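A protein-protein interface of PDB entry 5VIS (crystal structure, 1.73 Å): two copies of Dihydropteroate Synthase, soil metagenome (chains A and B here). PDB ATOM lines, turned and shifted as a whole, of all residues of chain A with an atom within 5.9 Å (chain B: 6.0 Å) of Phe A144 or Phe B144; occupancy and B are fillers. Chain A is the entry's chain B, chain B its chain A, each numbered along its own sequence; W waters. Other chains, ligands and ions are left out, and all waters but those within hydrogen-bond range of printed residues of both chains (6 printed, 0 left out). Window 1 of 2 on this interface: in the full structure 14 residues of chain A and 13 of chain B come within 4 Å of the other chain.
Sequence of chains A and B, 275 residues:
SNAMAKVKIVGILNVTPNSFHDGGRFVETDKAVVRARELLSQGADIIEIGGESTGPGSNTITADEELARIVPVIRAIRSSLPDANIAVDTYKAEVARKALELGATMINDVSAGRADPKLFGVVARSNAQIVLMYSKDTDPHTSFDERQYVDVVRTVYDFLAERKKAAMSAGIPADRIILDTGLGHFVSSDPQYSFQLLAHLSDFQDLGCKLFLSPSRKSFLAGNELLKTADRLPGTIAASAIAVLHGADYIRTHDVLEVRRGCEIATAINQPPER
Water W6 lies within hydrogen-bond range of O of Phe B144 (2.6 Å), N of Glu A146 (3.0 Å) and OD1 of Asp A145 (3.3 Å). Water W1 lies within hydrogen-bond range of O of Phe A144, N of Glu B146 and OD1 of Asp B145. Water W2 lies within hydrogen-bond range of OE2 of Glu B146, N of Gly A57 and O of Thr A142. Water W5 lies within hydrogen-bond range of O of Ser A189 (2.8 Å) and N of Gly B57 (3.5 Å). Water W4 lies within hydrogen-bond range of the side-chain carboxylate of Glu A146 (2.8 Å), the backbone carbonyl oxygen of Thr B142 (2.9 Å) and the backbone NH of Gly B57 (3.0 Å). Water W3 lies within hydrogen-bond range of the side-chain carboxylate of Asp B145 (2.8 Å) and the side-chain carboxylate of Asp A145 (3.0 Å).
Hydrophobic or aromatic side chains of chain B within 4 Å of the printed part of chain A: Phe B144. Of the 12 printed residues of chain A, 5 touch a printed residue of chain B. Among the printed residues, 9 pairs touch across the chains.
N of Phe B144 is in hydrogen-bond range of OE2 of Glu A146 (2.8 Å). The side-chain carboxylate (OE2) of Glu B146 lies within hydrogen-bond range of the backbone NH (N) of Phe A144 (2.9 Å).
Phe A144 touches four residues of chain B. Of chain A, only Phe A144 (3.4 Å), Asp A145 (3.6 Å), Glu A146 (2.8 Å) and Ser A189 (3.5 Å) come within 4 Å of Phe B144. Of the printed residues of chain B, Ser A189 touches Phe B144. Of the printed residues of chain B, Asp A145 touches Phe B144. Gly B57 touches none of the printed residues of chain A. Lys A136 touches none of the printed residues of chain B. The nearest residue of chain B that does not touch Phe A144 is His B185 (4.04 Å).
Among the printed residues, pairs that only touch across the chains: Glu A146 with Ser B143 (3.3 Å), Ser A143 with Glu B146 (3.4 Å), Phe A144 with Phe B144 (3.4 Å), Ser A189 with Phe B144 (3.5 Å), Phe A144 with Ser B189 (3.5 Å), Asp A145 with Phe B144 (3.6 Å) and Phe A144 with Asp B145 (3.8 Å).
Ser A143 touches Glu B146, and with the chains exchanged Glu A146 touches Ser B143. Phe B144 touches its own counterpart, Phe A144. Phe A144 touches Glu B146, and with the chains exchanged Glu A146 touches Phe B144. Phe A144 touches Ser B189, and with the chains exchanged Ser A189 touches Phe B144. 12 positions are printed for both chains. Of the 9 pairs that touch across the chains among the printed residues, 9 have their exchanged pair printed and touching as well.
O of Ser B143 lies within hydrogen-bond range of NZ of Lys B136, at 2.8 Å. O of Asp B145 lies within hydrogen-bond range of N of Ser B189 (2.9 Å). A ring nitrogen (ND1) of His B185 lies within hydrogen-bond range of the side-chain hydroxyl of Ser B189 (2.7 Å). The side-chain amino group of Lys A136 is in hydrogen-bond range of the backbone carbonyl oxygen of Ser A143, 2.8 Å away. OG of Ser A189 sits at hydrogen-bond distance from N of Asp A145, 2.9 Å away. A ring nitrogen (ND1) of His A185 lies within hydrogen-bond range of the side-chain hydroxyl of Ser A189 (2.8 Å).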
ATOM      1  N   PRO A  56      18.594  -7.344 -22.822  1.00  0.00           N
ATOM      2  CA  PRO A  56      19.036  -7.220 -21.430  1.00  0.00           C
ATOM      3  C   PRO A  56      18.610  -8.384 -20.564  1.00  0.00           C
ATOM      4  O   PRO A  56      17.470  -8.864 -20.667  1.00  0.00           O
ATOM      5  CB  PRO A  56      18.426  -5.897 -20.943  1.00  0.00           C
ATOM      6  CG  PRO A  56      17.669  -5.338 -22.064  1.00  0.00           C
ATOM      7  CD  PRO A  56      17.690  -6.272 -23.245  1.00  0.00           C
ATOM      8  N   GLY A  57      19.551  -8.848 -19.744  1.00  0.00           N
ATOM      9  CA  GLY A  57      19.344  -9.980 -18.851  1.00  0.00           C
ATOM     10  C   GLY A  57      19.723 -11.305 -19.479  1.00  0.00           C
ATOM     11  O   GLY A  57      19.738 -12.316 -18.790  1.00  0.00           O
ATOM     12  N   LYS A 136      25.965  -0.452 -27.921  1.00  0.00           N
ATOM     13  CA  LYS A 136      26.771   0.334 -26.987  1.00  0.00           C
ATOM     14  C   LYS A 136      27.729  -0.536 -26.164  1.00  0.00           C
ATOM     15  O   LYS A 136      28.616  -0.019 -25.496  1.00  0.00           O
ATOM     16  CB  LYS A 136      25.849   1.062 -26.010  1.00  0.00           C
ATOM     17  CG  LYS A 136      25.141   0.130 -25.039  1.00  0.00           C
ATOM     18  CD  LYS A 136      24.026   0.831 -24.292  1.00  0.00           C
ATOM     19  CE  LYS A 136      23.532  -0.012 -23.124  1.00  0.00           C
ATOM     20  NZ  LYS A 136      23.077  -1.362 -23.530  1.00  0.00           N
ATOM     21  N   THR A 142      23.328  -7.390 -24.536  1.00  0.00           N
ATOM     22  CA  THR A 142      23.288  -5.982 -24.158  1.00  0.00           C
ATOM     23  C   THR A 142      22.892  -5.758 -22.716  1.00  0.00           C
ATOM     24  O   THR A 142      22.198  -6.568 -22.115  1.00  0.00           O
ATOM     25  CB  THR A 142      22.414  -5.146 -25.128  1.00  0.00           C
ATOM     26  OG1 THR A 142      22.877  -3.788 -25.150  1.00  0.00           O
ATOM     27  CG2 THR A 142      20.965  -5.215 -24.801  1.00  0.00           C
ATOM     28  N   SER A 143      23.347  -4.653 -22.164  1.00  0.00           N
ATOM     29  CA  SER A 143      23.083  -4.344 -20.762  1.00  0.00           C
ATOM     30  C   SER A 143      21.959  -3.351 -20.541  1.00  0.00           C
ATOM     31  O   SER A 143      21.598  -2.601 -21.444  1.00  0.00           O
ATOM     32  CB  SER A 143      24.337  -3.702 -20.176  1.00  0.00           C
ATOM     33  OG  SER A 143      24.645  -2.505 -20.898  1.00  0.00           O
ATOM     34  N   PHE A 144      21.413  -3.374 -19.327  1.00  0.00           N
ATOM     35  CA  PHE A 144      20.479  -2.340 -18.898  1.00  0.00           C
ATOM     36  C   PHE A 144      21.434  -1.192 -18.502  1.00  0.00           C
ATOM     37  O   PHE A 144      22.222  -1.337 -17.537  1.00  0.00           O
ATOM     38  CB  PHE A 144      19.703  -2.739 -17.657  1.00  0.00           C
ATOM     39  CG  PHE A 144      18.552  -3.676 -17.892  1.00  0.00           C
ATOM     40  CD1 PHE A 144      17.413  -3.219 -18.527  1.00  0.00           C
ATOM     41  CD2 PHE A 144      18.558  -4.958 -17.372  1.00  0.00           C
ATOM     42  CE1 PHE A 144      16.315  -4.059 -18.697  1.00  0.00           C
ATOM     43  CE2 PHE A 144      17.469  -5.793 -17.533  1.00  0.00           C
ATOM     44  CZ  PHE A 144      16.349  -5.341 -18.198  1.00  0.00           C
ATOM     45  N   ASP A 145      21.384  -0.071 -19.212  1.00  0.00           N
ATOM     46  CA  ASP A 145      22.287   1.052 -18.940  1.00  0.00           C
ATOM     47  C   ASP A 145      21.741   2.268 -19.659  1.00  0.00           C
ATOM     48  O   ASP A 145      21.582   2.232 -20.873  1.00  0.00           O
ATOM     49  CB  ASP A 145      23.696   0.695 -19.456  1.00  0.00           C
ATOM     50  CG  ASP A 145      24.704   1.858 -19.394  1.00  0.00           C
ATOM     51  OD1 ASP A 145      24.428   2.920 -18.832  1.00  0.00           O
ATOM     52  OD2 ASP A 145      25.816   1.680 -19.934  1.00  0.00           O
ATOM     53  N   GLU A 146      21.455   3.340 -18.910  1.00  0.00           N
ATOM     54  CA  GLU A 146      20.947   4.587 -19.501  1.00  0.00           C
ATOM     55  C   GLU A 146      22.091   5.400 -20.061  1.00  0.00           C
ATOM     56  O   GLU A 146      22.348   6.535 -19.640  1.00  0.00           O
ATOM     57  CB  GLU A 146      20.161   5.390 -18.479  1.00  0.00           C
ATOM     58  CG  GLU A 146      18.897   4.674 -18.092  1.00  0.00           C
ATOM     59  CD  GLU A 146      18.115   5.379 -17.012  1.00  0.00           C
ATOM     60  OE1 GLU A 146      18.432   6.526 -16.649  1.00  0.00           O
ATOM     61  OE2 GLU A 146      17.178   4.746 -16.528  1.00  0.00           O
ATOM     62  N   HIS A 185      17.486  -0.860 -26.139  1.00  0.00           N
ATOM     63  CA  HIS A 185      18.610  -1.022 -25.199  1.00  0.00           C
ATOM     64  C   HIS A 185      19.989  -1.099 -25.839  1.00  0.00           C
ATOM     65  O   HIS A 185      20.974  -0.663 -25.228  1.00  0.00           O
ATOM     66  CB  HIS A 185      18.377  -2.220 -24.252  1.00  0.00           C
ATOM     67  CG  HIS A 185      17.212  -2.053 -23.329  1.00  0.00           C
ATOM     68  ND1 HIS A 185      17.269  -1.246 -22.219  1.00  0.00           N
ATOM     69  CD2 HIS A 185      15.986  -2.634 -23.310  1.00  0.00           C
ATOM     70  CE1 HIS A 185      16.125  -1.308 -21.562  1.00  0.00           C
ATOM     71  NE2 HIS A 185      15.327  -2.146 -22.203  1.00  0.00           N
ATOM     72  N   SER A 189      19.272   2.446 -22.706  1.00  0.00           N
ATOM     73  CA  SER A 189      18.030   2.194 -21.966  1.00  0.00           C
ATOM     74  C   SER A 189      17.257   3.534 -21.833  1.00  0.00           C
ATOM     75  O   SER A 189      16.121   3.557 -21.346  1.00  0.00           O
ATOM     76  CB  SER A 189      18.308   1.553 -20.616  1.00  0.00           C
ATOM     77  OG  SER A 189      19.009   0.328 -20.782  1.00  0.00           O
ATOM     78  N   ASP A 190      17.891   4.648 -22.214  1.00  0.00           N
ATOM     79  CA  ASP A 190      17.223   5.964 -22.270  1.00  0.00           C
ATOM     80  C   ASP A 190      16.608   6.017 -23.684  1.00  0.00           C
ATOM     81  O   ASP A 190      17.348   6.038 -24.683  1.00  0.00           O
ATOM     82  CB  ASP A 190      18.207   7.121 -22.041  1.00  0.00           C
ATOM     83  CG  ASP A 190      17.549   8.502 -22.153  1.00  0.00           C
ATOM     84  OD1 ASP A 190      16.424   8.616 -22.725  1.00  0.00           O
ATOM     85  OD2 ASP A 190      18.168   9.500 -21.671  1.00  0.00           O
ATOM     86  N   SER A 219      11.088  -1.552 -25.736  1.00  0.00           N
ATOM     87  CA  SER A 219      10.665  -0.667 -24.639  1.00  0.00           C
ATOM     88  C   SER A 219      10.857   0.830 -24.863  1.00  0.00           C
ATOM     89  O   SER A 219      10.212   1.623 -24.165  1.00  0.00           O
ATOM     90  CB  SER A 219      11.276  -1.107 -23.320  1.00  0.00           C
ATOM     91  OG  SER A 219      12.673  -1.057 -23.376  1.00  0.00           O
ATOM     92  N   PRO B  56      12.116   3.053 -13.802  1.00  0.00           N
ATOM     93  CA  PRO B  56      13.018   3.534 -14.844  1.00  0.00           C
ATOM     94  C   PRO B  56      12.267   4.038 -16.086  1.00  0.00           C
ATOM     95  O   PRO B  56      11.241   3.475 -16.457  1.00  0.00           O
ATOM     96  CB  PRO B  56      13.901   2.317 -15.141  1.00  0.00           C
ATOM     97  CG  PRO B  56      13.176   1.148 -14.606  1.00  0.00           C
ATOM     98  CD  PRO B  56      12.282   1.621 -13.512  1.00  0.00           C
ATOM     99  N   GLY B  57      12.776   5.109 -16.681  1.00  0.00           N
ATOM    100  CA  GLY B  57      12.171   5.738 -17.864  1.00  0.00           C
ATOM    101  C   GLY B  57      11.097   6.765 -17.507  1.00  0.00           C
ATOM    102  O   GLY B  57      10.716   7.577 -18.351  1.00  0.00           O
ATOM    103  N   LYS B 136      19.025   2.486  -4.942  1.00  0.00           N
ATOM    104  CA  LYS B 136      20.443   2.628  -5.234  1.00  0.00           C
ATOM    105  C   LYS B 136      20.785   4.051  -5.745  1.00  0.00           C
ATOM    106  O   LYS B 136      21.952   4.420  -5.824  1.00  0.00           O
ATOM    107  CB  LYS B 136      20.829   1.621  -6.300  1.00  0.00           C
ATOM    108  CG  LYS B 136      20.286   1.964  -7.672  1.00  0.00           C
ATOM    109  CD  LYS B 136      20.393   0.793  -8.637  1.00  0.00           C
ATOM    110  CE  LYS B 136      20.069   1.231 -10.060  1.00  0.00           C
ATOM    111  NZ  LYS B 136      18.722   1.871 -10.169  1.00  0.00           N
ATOM    112  N   THR B 142      14.292   6.005 -10.447  1.00  0.00           N
ATOM    113  CA  THR B 142      15.388   5.061 -10.500  1.00  0.00           C
ATOM    114  C   THR B 142      15.886   4.841 -11.936  1.00  0.00           C
ATOM    115  O   THR B 142      15.163   5.049 -12.899  1.00  0.00           O
ATOM    116  CB  THR B 142      15.007   3.729  -9.805  1.00  0.00           C
ATOM    117  OG1 THR B 142      16.188   3.054  -9.366  1.00  0.00           O
ATOM    118  CG2 THR B 142      14.187   2.857 -10.668  1.00  0.00           C
ATOM    119  N   SER B 143      17.139   4.443 -12.048  1.00  0.00           N
ATOM    120  CA  SER B 143      17.770   4.221 -13.330  1.00  0.00           C
ATOM    121  C   SER B 143      17.932   2.761 -13.708  1.00  0.00           C
ATOM    122  O   SER B 143      17.901   1.875 -12.848  1.00  0.00           O
ATOM    123  CB  SER B 143      19.169   4.794 -13.262  1.00  0.00           C
ATOM    124  OG  SER B 143      19.914   4.154 -12.232  1.00  0.00           O
ATOM    125  N   PHE B 144      18.058   2.514 -15.011  1.00  0.00           N
ATOM    126  CA  PHE B 144      18.432   1.178 -15.482  1.00  0.00           C
ATOM    127  C   PHE B 144      19.961   1.171 -15.257  1.00  0.00           C
ATOM    128  O   PHE B 144      20.691   1.973 -15.868  1.00  0.00           O
ATOM    129  CB  PHE B 144      18.181   0.981 -16.967  1.00  0.00           C
ATOM    130  CG  PHE B 144      16.739   0.828 -17.354  1.00  0.00           C
ATOM    131  CD1 PHE B 144      16.090  -0.376 -17.169  1.00  0.00           C
ATOM    132  CD2 PHE B 144      16.064   1.859 -17.998  1.00  0.00           C
ATOM    133  CE1 PHE B 144      14.776  -0.550 -17.575  1.00  0.00           C
ATOM    134  CE2 PHE B 144      14.746   1.695 -18.406  1.00  0.00           C
ATOM    135  CZ  PHE B 144      14.108   0.486 -18.191  1.00  0.00           C
ATOM    136  N   ASP B 145      20.453   0.260 -14.415  1.00  0.00           N
ATOM    137  CA  ASP B 145      21.868   0.176 -14.094  1.00  0.00           C
ATOM    138  C   ASP B 145      22.136  -1.155 -13.408  1.00  0.00           C
ATOM    139  O   ASP B 145      21.489  -1.462 -12.398  1.00  0.00           O
ATOM    140  CB  ASP B 145      22.253   1.335 -13.153  1.00  0.00           C
ATOM    141  CG  ASP B 145      23.708   1.278 -12.711  1.00  0.00           C
ATOM    142  OD1 ASP B 145      24.572   0.807 -13.484  1.00  0.00           O
ATOM    143  OD2 ASP B 145      24.000   1.734 -11.587  1.00  0.00           O
ATOM    144  N   GLU B 146      23.064  -1.942 -13.949  1.00  0.00           N
ATOM    145  CA  GLU B 146      23.394  -3.265 -13.390  1.00  0.00           C
ATOM    146  C   GLU B 146      24.376  -3.143 -12.221  1.00  0.00           C
ATOM    147  O   GLU B 146      25.464  -3.721 -12.226  1.00  0.00           O
ATOM    148  CB  GLU B 146      23.887  -4.214 -14.494  1.00  0.00           C
ATOM    149  CG  GLU B 146      22.831  -4.426 -15.582  1.00  0.00           C
ATOM    150  CD  GLU B 146      23.256  -5.321 -16.738  1.00  0.00           C
ATOM    151  OE1 GLU B 146      24.402  -5.817 -16.761  1.00  0.00           O
ATOM    152  OE2 GLU B 146      22.421  -5.530 -17.653  1.00  0.00           O
ATOM    153  N   HIS B 185      14.794  -2.894 -10.309  1.00  0.00           N
ATOM    154  CA  HIS B 185      15.740  -1.842 -10.666  1.00  0.00           C
ATOM    155  C   HIS B 185      16.132  -0.907  -9.523  1.00  0.00           C
ATOM    156  O   HIS B 185      17.228  -0.369  -9.542  1.00  0.00           O
ATOM    157  CB  HIS B 185      15.274  -1.036 -11.885  1.00  0.00           C
ATOM    158  CG  HIS B 185      15.073  -1.864 -13.118  1.00  0.00           C
ATOM    159  ND1 HIS B 185      16.118  -2.459 -13.795  1.00  0.00           N
ATOM    160  CD2 HIS B 185      13.949  -2.190 -13.798  1.00  0.00           C
ATOM    161  CE1 HIS B 185      15.639  -3.136 -14.827  1.00  0.00           C
ATOM    162  NE2 HIS B 185      14.328  -2.958 -14.869  1.00  0.00           N
ATOM    163  N   SER B 189      19.593  -3.527 -11.773  1.00  0.00           N
ATOM    164  CA  SER B 189      19.079  -4.142 -13.000  1.00  0.00           C
ATOM    165  C   SER B 189      19.613  -5.582 -13.150  1.00  0.00           C
ATOM    166  O   SER B 189      19.186  -6.319 -14.065  1.00  0.00           O
ATOM    167  CB  SER B 189      19.398  -3.281 -14.211  1.00  0.00           C
ATOM    168  OG  SER B 189      18.738  -2.034 -14.086  1.00  0.00           O
ATOM    169  N   ASP B 190      20.569  -5.968 -12.285  1.00  0.00           N
ATOM    170  CA  ASP B 190      21.060  -7.345 -12.220  1.00  0.00           C
ATOM    171  C   ASP B 190      20.089  -8.029 -11.227  1.00  0.00           C
ATOM    172  O   ASP B 190      20.055  -7.661 -10.035  1.00  0.00           O
ATOM    173  CB  ASP B 190      22.497  -7.393 -11.715  1.00  0.00           C
ATOM    174  CG  ASP B 190      23.026  -8.809 -11.521  1.00  0.00           C
ATOM    175  OD1 ASP B 190      22.242  -9.793 -11.463  1.00  0.00           O
ATOM    176  OD2 ASP B 190      24.263  -8.941 -11.397  1.00  0.00           O
ATOM    177  N   SER B 219      11.208  -6.506 -13.168  1.00  0.00           N
ATOM    178  CA  SER B 219      12.298  -6.956 -13.993  1.00  0.00           C
ATOM    179  C   SER B 219      12.996  -8.235 -13.562  1.00  0.00           C
ATOM    180  O   SER B 219      13.261  -9.127 -14.382  1.00  0.00           O
ATOM    181  CB  SER B 219      13.341  -5.823 -13.962  1.00  0.00           C
ATOM    182  OG  SER B 219      13.628  -5.455 -12.608  1.00  0.00           O
HETATM  183  O   HOH W   1      24.526  -1.005 -16.230  1.00  0.00           O
HETATM  184  O   HOH W   2      22.076  -7.747 -19.202  1.00  0.00           O
HETATM  185  O   HOH W   3      24.933   1.976 -15.989  1.00  0.00           O
HETATM  186  O   HOH W   4      15.183   6.377 -15.523  1.00  0.00           O
HETATM  187  O   HOH W   5      15.058   5.068 -19.308  1.00  0.00           O
HETATM  188  O   HOH W   6      22.626   3.715 -16.152  1.00  0.00           O
